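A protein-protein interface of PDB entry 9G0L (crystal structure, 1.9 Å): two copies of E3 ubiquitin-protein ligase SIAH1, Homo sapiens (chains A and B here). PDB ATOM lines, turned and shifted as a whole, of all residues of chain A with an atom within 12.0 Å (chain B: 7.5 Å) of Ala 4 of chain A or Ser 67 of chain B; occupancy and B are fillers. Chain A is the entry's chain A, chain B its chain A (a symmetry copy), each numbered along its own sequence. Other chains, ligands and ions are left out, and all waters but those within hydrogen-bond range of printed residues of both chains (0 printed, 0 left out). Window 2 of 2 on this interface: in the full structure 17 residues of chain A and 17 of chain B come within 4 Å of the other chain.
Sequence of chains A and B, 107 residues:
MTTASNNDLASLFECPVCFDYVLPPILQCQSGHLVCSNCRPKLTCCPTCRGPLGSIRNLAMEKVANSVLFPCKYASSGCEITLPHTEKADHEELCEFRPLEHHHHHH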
ATOM      1  N   THR A   3     -23.248  18.260  15.244  1.00  0.00           N
ATOM      2  CA  THR A   3     -23.939  16.984  15.090  1.00  0.00           C
ATOM      3  C   THR A   3     -23.010  15.795  15.304  1.00  0.00           C
ATOM      4  O   THR A   3     -22.178  15.789  16.211  1.00  0.00           O
ATOM      5  CB  THR A   3     -24.576  16.852  13.690  1.00  0.00           C
ATOM      6  N   ALA A   4     -23.168  14.790  14.447  1.00  0.00           N
ATOM      7  CA  ALA A   4     -22.396  13.559  14.491  1.00  0.00           C
ATOM      8  C   ALA A   4     -21.008  13.754  13.887  1.00  0.00           C
ATOM      9  O   ALA A   4     -20.788  14.621  13.038  1.00  0.00           O
ATOM     10  CB  ALA A   4     -23.121  12.460  13.732  1.00  0.00           C
ATOM     11  N   SER A   5     -20.072  12.905  14.313  1.00  0.00           N
ATOM     12  CA  SER A   5     -18.677  13.008  13.900  1.00  0.00           C
ATOM     13  C   SER A   5     -18.199  11.680  13.332  1.00  0.00           C
ATOM     14  O   SER A   5     -18.819  10.634  13.531  1.00  0.00           O
ATOM     15  CB  SER A   5     -17.767  13.422  15.069  1.00  0.00           C
ATOM     16  OG  SER A   5     -17.200  12.280  15.697  1.00  0.00           O
ATOM     17  N   ASN A   6     -17.072  11.737  12.618  1.00  0.00           N
ATOM     18  CA  ASN A   6     -16.477  10.511  12.092  1.00  0.00           C
ATOM     19  C   ASN A   6     -16.016   9.595  13.219  1.00  0.00           C
ATOM     20  O   ASN A   6     -16.260   8.384  13.178  1.00  0.00           O
ATOM     21  CB  ASN A   6     -15.310  10.841  11.159  1.00  0.00           C
ATOM     22  CG  ASN A   6     -14.574   9.601  10.681  1.00  0.00           C
ATOM     23  OD1 ASN A   6     -15.019   8.914   9.764  1.00  0.00           O
ATOM     24  ND2 ASN A   6     -13.452   9.297  11.320  1.00  0.00           N
ATOM     25  N   ASN A   7     -15.353  10.145  14.240  1.00  0.00           N
ATOM     26  CA  ASN A   7     -14.882   9.294  15.330  1.00  0.00           C
ATOM     27  C   ASN A   7     -16.041   8.673  16.105  1.00  0.00           C
ATOM     28  O   ASN A   7     -15.902   7.565  16.637  1.00  0.00           O
ATOM     29  CB  ASN A   7     -13.963  10.082  16.262  1.00  0.00           C
ATOM     30  CG  ASN A   7     -13.127  11.112  15.522  1.00  0.00           C
ATOM     31  OD1 ASN A   7     -13.657  12.042  14.897  1.00  0.00           O
ATOM     32  ND2 ASN A   7     -11.811  10.928  15.553  1.00  0.00           N
ATOM     33  N   ASP A   8     -17.191   9.351  16.157  1.00  0.00           N
ATOM     34  CA  ASP A   8     -18.372   8.750  16.769  1.00  0.00           C
ATOM     35  C   ASP A   8     -18.817   7.521  15.988  1.00  0.00           C
ATOM     36  O   ASP A   8     -19.112   6.475  16.577  1.00  0.00           O
ATOM     37  CB  ASP A   8     -19.517   9.765  16.866  1.00  0.00           C
ATOM     38  CG  ASP A   8     -19.209  10.920  17.811  1.00  0.00           C
ATOM     39  OD1 ASP A   8     -18.468  10.718  18.798  1.00  0.00           O
ATOM     40  OD2 ASP A   8     -19.736  12.029  17.578  1.00  0.00           O
ATOM     41  N   LEU A   9     -18.862   7.624  14.653  1.00  0.00           N
ATOM     42  CA  LEU A   9     -19.249   6.477  13.838  1.00  0.00           C
ATOM     43  C   LEU A   9     -18.208   5.374  13.920  1.00  0.00           C
ATOM     44  O   LEU A   9     -18.548   4.205  14.114  1.00  0.00           O
ATOM     45  CB  LEU A   9     -19.453   6.889  12.384  1.00  0.00           C
ATOM     46  CG  LEU A   9     -20.734   7.697  12.198  1.00  0.00           C
ATOM     47  CD1 LEU A   9     -20.876   8.119  10.765  1.00  0.00           C
ATOM     48  CD2 LEU A   9     -21.931   6.894  12.674  1.00  0.00           C
ATOM     49  N   ALA A  10     -16.930   5.723  13.762  1.00  0.00           N
ATOM     50  CA  ALA A  10     -15.901   4.696  13.810  1.00  0.00           C
ATOM     51  C   ALA A  10     -15.964   3.909  15.114  1.00  0.00           C
ATOM     52  O   ALA A  10     -15.815   2.689  15.109  1.00  0.00           O
ATOM     53  CB  ALA A  10     -14.524   5.314  13.619  1.00  0.00           C
ATOM     54  N   SER A  11     -16.195   4.578  16.242  1.00  0.00           N
ATOM     55  CA  SER A  11     -16.190   3.842  17.504  1.00  0.00           C
ATOM     56  C   SER A  11     -17.279   2.777  17.547  1.00  0.00           C
ATOM     57  O   SER A  11     -17.147   1.798  18.285  1.00  0.00           O
ATOM     58  CB  SER A  11     -16.343   4.802  18.682  1.00  0.00           C
ATOM     59  OG  SER A  11     -17.660   5.306  18.741  1.00  0.00           O
ATOM     60  N   LEU A  12     -18.331   2.919  16.744  1.00  0.00           N
ATOM     61  CA  LEU A  12     -19.359   1.889  16.711  1.00  0.00           C
ATOM     62  C   LEU A  12     -18.854   0.570  16.154  1.00  0.00           C
ATOM     63  O   LEU A  12     -19.533  -0.452  16.320  1.00  0.00           O
ATOM     64  CB  LEU A  12     -20.554   2.365  15.896  1.00  0.00           C
ATOM     65  CG  LEU A  12     -21.142   3.683  16.387  1.00  0.00           C
ATOM     66  CD1 LEU A  12     -22.239   4.113  15.457  1.00  0.00           C
ATOM     67  CD2 LEU A  12     -21.653   3.570  17.821  1.00  0.00           C
ATOM     68  N   PHE A  13     -17.691   0.566  15.511  1.00  0.00           N
ATOM     69  CA  PHE A  13     -17.102  -0.635  14.943  1.00  0.00           C
ATOM     70  C   PHE A  13     -16.045  -1.264  15.845  1.00  0.00           C
ATOM     71  O   PHE A  13     -15.414  -2.239  15.436  1.00  0.00           O
ATOM     72  CB  PHE A  13     -16.463  -0.325  13.577  1.00  0.00           C
ATOM     73  CG  PHE A  13     -17.435   0.124  12.505  1.00  0.00           C
ATOM     74  CD1 PHE A  13     -17.921   1.424  12.480  1.00  0.00           C
ATOM     75  CD2 PHE A  13     -17.835  -0.750  11.508  1.00  0.00           C
ATOM     76  CE1 PHE A  13     -18.808   1.834  11.491  1.00  0.00           C
ATOM     77  CE2 PHE A  13     -18.706  -0.349  10.512  1.00  0.00           C
ATOM     78  CZ  PHE A  13     -19.194   0.940  10.496  1.00  0.00           C
ATOM     79  N   MET A  61     -24.257  -2.209   8.414  1.00  0.00           N
ATOM     80  CA  MET A  61     -23.008  -1.707   8.987  1.00  0.00           C
ATOM     81  C   MET A  61     -21.871  -1.693   7.982  1.00  0.00           C
ATOM     82  O   MET A  61     -21.023  -0.791   8.028  1.00  0.00           O
ATOM     83  CB  MET A  61     -22.642  -2.566  10.188  1.00  0.00           C
ATOM     84  CG  MET A  61     -23.159  -2.077  11.528  1.00  0.00           C
ATOM     85  SD  MET A  61     -23.261  -0.269  11.837  1.00  0.00           S
ATOM     86  CE  MET A  61     -21.674  -0.006  12.552  1.00  0.00           C
ATOM     87  N   VAL A  64     -22.469   1.466   6.079  1.00  0.00           N
ATOM     88  CA  VAL A  64     -21.995   2.581   6.899  1.00  0.00           C
ATOM     89  C   VAL A  64     -20.486   2.683   6.832  1.00  0.00           C
ATOM     90  O   VAL A  64     -19.923   3.782   6.772  1.00  0.00           O
ATOM     91  CB  VAL A  64     -22.461   2.428   8.358  1.00  0.00           C
ATOM     92  CG1 VAL A  64     -21.868   3.543   9.246  1.00  0.00           C
ATOM     93  CG2 VAL A  64     -23.984   2.424   8.421  1.00  0.00           C
ATOM     94  N   ALA A  65     -19.802   1.538   6.869  1.00  0.00           N
ATOM     95  CA  ALA A  65     -18.345   1.558   6.921  1.00  0.00           C
ATOM     96  C   ALA A  65     -17.747   2.254   5.706  1.00  0.00           C
ATOM     97  O   ALA A  65     -16.681   2.868   5.825  1.00  0.00           O
ATOM     98  CB  ALA A  65     -17.804   0.139   7.057  1.00  0.00           C
ATOM     99  N   SER A  67     -18.514   4.968   4.693  1.00  0.00           N
ATOM    100  CA  SER A  67     -18.607   6.397   4.970  1.00  0.00           C
ATOM    101  C   SER A  67     -17.725   6.831   6.135  1.00  0.00           C
ATOM    102  O   SER A  67     -17.868   7.959   6.625  1.00  0.00           O
ATOM    103  CB  SER A  67     -20.060   6.781   5.259  1.00  0.00           C
ATOM    104  OG  SER A  67     -20.908   6.486   4.167  1.00  0.00           O
ATOM    105  N   VAL A  68     -16.815   5.974   6.583  1.00  0.00           N
ATOM    106  CA  VAL A  68     -16.071   6.188   7.816  1.00  0.00           C
ATOM    107  C   VAL A  68     -14.588   6.097   7.497  1.00  0.00           C
ATOM    108  O   VAL A  68     -14.162   5.224   6.732  1.00  0.00           O
ATOM    109  CB  VAL A  68     -16.476   5.140   8.881  1.00  0.00           C
ATOM    110  CG1 VAL A  68     -15.530   5.157  10.058  1.00  0.00           C
ATOM    111  CG2 VAL A  68     -17.908   5.364   9.329  1.00  0.00           C
ATOM    112  N   LEU A  69     -13.804   6.988   8.085  1.00  0.00           N
ATOM    113  CA  LEU A  69     -12.354   6.897   8.055  1.00  0.00           C
ATOM    114  C   LEU A  69     -11.902   6.271   9.369  1.00  0.00           C
ATOM    115  O   LEU A  69     -12.200   6.802  10.443  1.00  0.00           O
ATOM    116  CB  LEU A  69     -11.733   8.281   7.862  1.00  0.00           C
ATOM    117  CG  LEU A  69     -12.087   8.934   6.525  1.00  0.00           C
ATOM    118  CD1 LEU A  69     -11.686  10.400   6.494  1.00  0.00           C
ATOM    119  CD2 LEU A  69     -11.498   8.178   5.332  1.00  0.00           C
ATOM    120  N   SER B   5     -21.998  11.927   3.764  1.00  0.00           N
ATOM    121  CA  SER B   5     -23.045  12.910   4.014  1.00  0.00           C
ATOM    122  C   SER B   5     -24.142  12.303   4.875  1.00  0.00           C
ATOM    123  O   SER B   5     -24.246  11.082   5.018  1.00  0.00           O
ATOM    124  CB  SER B   5     -23.654  13.436   2.703  1.00  0.00           C
ATOM    125  OG  SER B   5     -24.821  12.701   2.358  1.00  0.00           O
ATOM    126  N   ASN B   6     -24.971  13.178   5.447  1.00  0.00           N
ATOM    127  CA  ASN B   6     -26.109  12.704   6.231  1.00  0.00           C
ATOM    128  C   ASN B   6     -27.104  11.951   5.355  1.00  0.00           C
ATOM    129  O   ASN B   6     -27.589  10.883   5.741  1.00  0.00           O
ATOM    130  CB  ASN B   6     -26.796  13.875   6.936  1.00  0.00           C
ATOM    131  CG  ASN B   6     -28.062  13.458   7.665  1.00  0.00           C
ATOM    132  OD1 ASN B   6     -28.010  12.916   8.767  1.00  0.00           O
ATOM    133  ND2 ASN B   6     -29.208  13.687   7.038  1.00  0.00           N
ATOM    134  N   LEU B   9     -26.017   8.416   4.753  1.00  0.00           N
ATOM    135  CA  LEU B   9     -26.283   7.522   5.876  1.00  0.00           C
ATOM    136  C   LEU B   9     -27.769   7.235   6.005  1.00  0.00           C
ATOM    137  O   LEU B   9     -28.172   6.080   6.162  1.00  0.00           O
ATOM    138  CB  LEU B   9     -25.757   8.118   7.178  1.00  0.00           C
ATOM    139  CG  LEU B   9     -24.233   8.068   7.250  1.00  0.00           C
ATOM    140  CD1 LEU B   9     -23.755   8.701   8.524  1.00  0.00           C
ATOM    141  CD2 LEU B   9     -23.751   6.636   7.111  1.00  0.00           C
ATOM    142  N   PHE B  13     -31.061   3.362   5.725  1.00  0.00           N
ATOM    143  CA  PHE B  13     -32.176   2.915   6.542  1.00  0.00           C
ATOM    144  C   PHE B  13     -33.477   2.785   5.755  1.00  0.00           C
ATOM    145  O   PHE B  13     -34.512   2.494   6.355  1.00  0.00           O
ATOM    146  CB  PHE B  13     -32.406   3.886   7.714  1.00  0.00           C
ATOM    147  CG  PHE B  13     -31.264   3.971   8.706  1.00  0.00           C
ATOM    148  CD1 PHE B  13     -30.125   4.713   8.422  1.00  0.00           C
ATOM    149  CD2 PHE B  13     -31.347   3.331   9.931  1.00  0.00           C
ATOM    150  CE1 PHE B  13     -29.081   4.793   9.338  1.00  0.00           C
ATOM    151  CE2 PHE B  13     -30.321   3.416  10.854  1.00  0.00           C
ATOM    152  CZ  PHE B  13     -29.188   4.145  10.566  1.00  0.00           C
ATOM    153  N   MET B  61     -26.656  -0.622  13.843  1.00  0.00           N
ATOM    154  CA  MET B  61     -27.442   0.324  13.051  1.00  0.00           C
ATOM    155  C   MET B  61     -28.279   1.251  13.914  1.00  0.00           C
ATOM    156  O   MET B  61     -28.464   2.422  13.555  1.00  0.00           O
ATOM    157  CB  MET B  61     -28.332  -0.458  12.098  1.00  0.00           C
ATOM    158  CG  MET B  61     -27.747  -0.732  10.726  1.00  0.00           C
ATOM    159  SD  MET B  61     -26.662   0.534   9.952  1.00  0.00           S
ATOM    160  CE  MET B  61     -27.873   1.448   9.060  1.00  0.00           C
ATOM    161  N   GLU B  62     -28.865   0.738  15.008  1.00  0.00           N
ATOM    162  CA  GLU B  62     -29.568   1.633  15.927  1.00  0.00           C
ATOM    163  C   GLU B  62     -28.631   2.687  16.473  1.00  0.00           C
ATOM    164  O   GLU B  62     -29.037   3.835  16.687  1.00  0.00           O
ATOM    165  CB  GLU B  62     -30.199   0.860  17.081  1.00  0.00           C
ATOM    166  CG  GLU B  62     -31.289  -0.115  16.646  1.00  0.00           C
ATOM    167  CD  GLU B  62     -31.785  -0.983  17.798  1.00  0.00           C
ATOM    168  OE1 GLU B  62     -31.444  -0.718  18.972  1.00  0.00           O
ATOM    169  OE2 GLU B  62     -32.515  -1.937  17.528  1.00  0.00           O
ATOM    170  N   LYS B  63     -27.376   2.324  16.730  1.00  0.00           N
ATOM    171  CA  LYS B  63     -26.453   3.328  17.250  1.00  0.00           C
ATOM    172  C   LYS B  63     -26.071   4.343  16.175  1.00  0.00           C
ATOM    173  O   LYS B  63     -25.957   5.542  16.461  1.00  0.00           O
ATOM    174  CB  LYS B  63     -25.210   2.669  17.837  1.00  0.00           C
ATOM    175  CG  LYS B  63     -25.509   2.001  19.195  1.00  0.00           C
ATOM    176  CD  LYS B  63     -24.348   1.213  19.744  1.00  0.00           C
ATOM    177  CE  LYS B  63     -24.803   0.370  20.949  1.00  0.00           C
ATOM    178  NZ  LYS B  63     -26.281   0.189  20.916  1.00  0.00           N
ATOM    179  N   VAL B  64     -25.830   3.879  14.943  1.00  0.00           N
ATOM    180  CA  VAL B  64     -25.654   4.796  13.816  1.00  0.00           C
ATOM    181  C   VAL B  64     -26.826   5.751  13.724  1.00  0.00           C
ATOM    182  O   VAL B  64     -26.656   6.942  13.437  1.00  0.00           O
ATOM    183  CB  VAL B  64     -25.485   4.020  12.497  1.00  0.00           C
ATOM    184  CG1 VAL B  64     -25.413   4.986  11.295  1.00  0.00           C
ATOM    185  CG2 VAL B  64     -24.246   3.135  12.569  1.00  0.00           C
ATOM    186  N   ALA B  65     -28.039   5.239  13.937  1.00  0.00           N
ATOM    187  CA  ALA B  65     -29.224   6.069  13.756  1.00  0.00           C
ATOM    188  C   ALA B  65     -29.214   7.277  14.683  1.00  0.00           C
ATOM    189  O   ALA B  65     -29.748   8.328  14.314  1.00  0.00           O
ATOM    190  CB  ALA B  65     -30.486   5.236  13.960  1.00  0.00           C
ATOM    191  N   ASN B  66     -28.586   7.172  15.869  1.00  0.00           N
ATOM    192  CA  ASN B  66     -28.448   8.343  16.746  1.00  0.00           C
ATOM    193  C   ASN B  66     -27.585   9.450  16.145  1.00  0.00           C
ATOM    194  O   ASN B  66     -27.461  10.510  16.760  1.00  0.00           O
ATOM    195  CB  ASN B  66     -27.836   7.957  18.102  1.00  0.00           C
ATOM    196  CG  ASN B  66     -28.616   6.869  18.819  1.00  0.00           C
ATOM    197  OD1 ASN B  66     -29.828   6.731  18.645  1.00  0.00           O
ATOM    198  ND2 ASN B  66     -27.913   6.073  19.622  1.00  0.00           N
ATOM    199  N   SER B  67     -26.957   9.223  14.993  1.00  0.00           N
ATOM    200  CA  SER B  67     -26.093  10.207  14.351  1.00  0.00           C
ATOM    201  C   SER B  67     -26.668  10.733  13.041  1.00  0.00           C
ATOM    202  O   SER B  67     -25.951  11.397  12.280  1.00  0.00           O
ATOM    203  CB  SER B  67     -24.710   9.602  14.095  1.00  0.00           C
ATOM    204  OG  SER B  67     -24.090   9.185  15.295  1.00  0.00           O
ATOM    205  N   VAL B  68     -27.938  10.464  12.763  1.00  0.00           N
ATOM    206  CA  VAL B  68     -28.531  10.722  11.459  1.00  0.00           C
ATOM    207  C   VAL B  68     -29.769  11.579  11.662  1.00  0.00           C
ATOM    208  O   VAL B  68     -30.548  11.348  12.593  1.00  0.00           O
ATOM    209  CB  VAL B  68     -28.886   9.390  10.754  1.00  0.00           C
ATOM    210  CG1 VAL B  68     -29.752   9.625   9.539  1.00  0.00           C
ATOM    211  CG2 VAL B  68     -27.625   8.631  10.386  1.00  0.00           C
ATOM    212  N   LEU B  69     -29.955  12.560  10.791  1.00  0.00           N
ATOM    213  CA  LEU B  69     -31.190  13.322  10.720  1.00  0.00           C
ATOM    214  C   LEU B  69     -32.028  12.738   9.589  1.00  0.00           C
ATOM    215  O   LEU B  69     -31.575  12.694   8.441  1.00  0.00           O
ATOM    216  CB  LEU B  69     -30.895  14.802  10.480  1.00  0.00           C
ATOM    217  CG  LEU B  69     -30.119  15.469  11.618  1.00  0.00           C
ATOM    218  CD1 LEU B  69     -29.612  16.845  11.219  1.00  0.00           C
ATOM    219  CD2 LEU B  69     -30.929  15.536  12.915  1.00  0.00           C
ATOM    220  N   PHE B  70     -33.245  12.268   9.915  1.00  0.00           N
ATOM    221  CA  PHE B  70     -34.088  11.561   8.952  1.00  0.00           C
ATOM    222  C   PHE B  70     -35.127  12.506   8.381  1.00  0.00           C
ATOM    223  O   PHE B  70     -35.776  13.225   9.150  1.00  0.00           O
ATOM    224  CB  PHE B  70     -34.783  10.386   9.626  1.00  0.00           C
ATOM    225  CG  PHE B  70     -33.850   9.295  10.025  1.00  0.00           C
ATOM    226  CD1 PHE B  70     -33.542   8.283   9.142  1.00  0.00           C
ATOM    227  CD2 PHE B  70     -33.253   9.303  11.276  1.00  0.00           C
ATOM    228  CE1 PHE B  70     -32.667   7.287   9.492  1.00  0.00           C
ATOM    229  CE2 PHE B  70     -32.369   8.306  11.634  1.00  0.00           C
ATOM    230  CZ  PHE B  70     -32.086   7.291  10.733  1.00  0.00           C
ATOM    231  N   PRO B  84     -34.033  14.015  14.243  1.00  0.00           N
ATOM    232  CA  PRO B  84     -33.577  12.836  14.980  1.00  0.00           C
ATOM    233  C   PRO B  84     -34.718  11.841  15.055  1.00  0.00           C
ATOM    234  O   PRO B  84     -35.895  12.213  15.058  1.00  0.00           O
ATOM    235  CB  PRO B  84     -33.219  13.387  16.367  1.00  0.00           C
ATOM    236  CG  PRO B  84     -33.170  14.906  16.195  1.00  0.00           C
ATOM    237  CD  PRO B  84     -34.119  15.212  15.095  1.00  0.00           C
ATOM    238  N   HIS B  85     -34.371  10.561  15.096  1.00  0.00           N
ATOM    239  CA  HIS B  85     -35.426   9.563  15.023  1.00  0.00           C
ATOM    240  C   HIS B  85     -36.364   9.653  16.218  1.00  0.00           C
ATOM    241  O   HIS B  85     -37.546   9.317  16.103  1.00  0.00           O
ATOM    242  CB  HIS B  85     -34.824   8.167  14.882  1.00  0.00           C
ATOM    243  CG  HIS B  85     -34.046   7.715  16.071  1.00  0.00           C
ATOM    244  ND1 HIS B  85     -34.604   6.957  17.076  1.00  0.00           N
ATOM    245  CD2 HIS B  85     -32.745   7.887  16.406  1.00  0.00           C
ATOM    246  CE1 HIS B  85     -33.686   6.700  17.992  1.00  0.00           C
ATOM    247  NE2 HIS B  85     -32.550   7.255  17.611  1.00  0.00           N
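Ala 4 of chain A touches Ser 67 of chain B. Leu 9 of chain A touches Leu 9 of chain B (CD1 to CD1, 3.7 Å). Leu 12 of chain A touches Lys 63 of chain B (CD2 to CB, 3.7 Å). Leu 12 of chain A touches Val 64 of chain B (CD1 to N, 3.6 Å). Met 61 of chain A touches Met 61 of chain B. CG2 of Val 64 of chain B touches SD of Met 61 of chain A, 3.6 Å away. Met 61 of chain B touches Val 64 of chain A.
Ala 4 of chain A touches just one residue of chain B: Ser 67 (3.3 Å). Of the printed residues of chain B, Leu 9 of chain A touches Leu 9 (3.7 Å). Of the printed residues of chain B, Met 61 of chain A touches Met 61 (3.96 Å) and Val 64 (3.6 Å). Of the printed residues of chain B, Val 64 of chain A touches Met 61. Val 68 of chain A touches none of the printed residues of chain B. No residue of chain A comes within 4 Å of Asn 6 of chain B. Of the printed residues of chain A, Leu 9 of chain B touches Leu 9 (3.7 Å). Printed residues of chain A within 4 Å of Lys 63 of chain B: Leu 12. No residue of chain A comes within 4 Å of Asn 66 of chain B. Ser 67 of chain B touches just one residue of chain A: Ala 4 (3.3 Å). The nearest residue of chain B that does not touch Ala 4 of chain A is Val 68 of chain B (5.3 Å). The nearest residue of chain A that does not touch Ser 67 of chain B is Leu 9 of chain A (4.1 Å). The nearest printed residue of chain A that does not touch Lys 63 of chain B is Leu 9 of chain A (5.7 Å).
Hydrophobic or aromatic side chains of chain A that line the printed part of chain B: Ala 4, Leu 9, Leu 12, Met 61 and Val 64. Of the 16 printed residues of chain B, 5 touch a printed residue of chain A. Hydrophobic or aromatic side chains of chain B within 4 Å of the printed part of chain A: Leu 9, Met 61 and Val 64. Among the printed residues, no Asp or Glu carboxylate lies within 4 Å of a Lys or Arg side-chain nitrogen of the other chain.
Leu 9 of chain A touches its own counterpart, Leu 9 of chain B. Met 61 of chain B touches its own counterpart, Met 61 of chain A. Met 61 of chain A touches Val 64 of chain B, and with the chains exchanged Val 64 of chain A touches Met 61 of chain B. Positions printed for both chains: 5, 6, 9, 13, 61, 64, 65, 67, 68 and 69. Of the 7 pairs that touch across the chains among the printed residues, 4 have their exchanged pair printed and touching as well.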
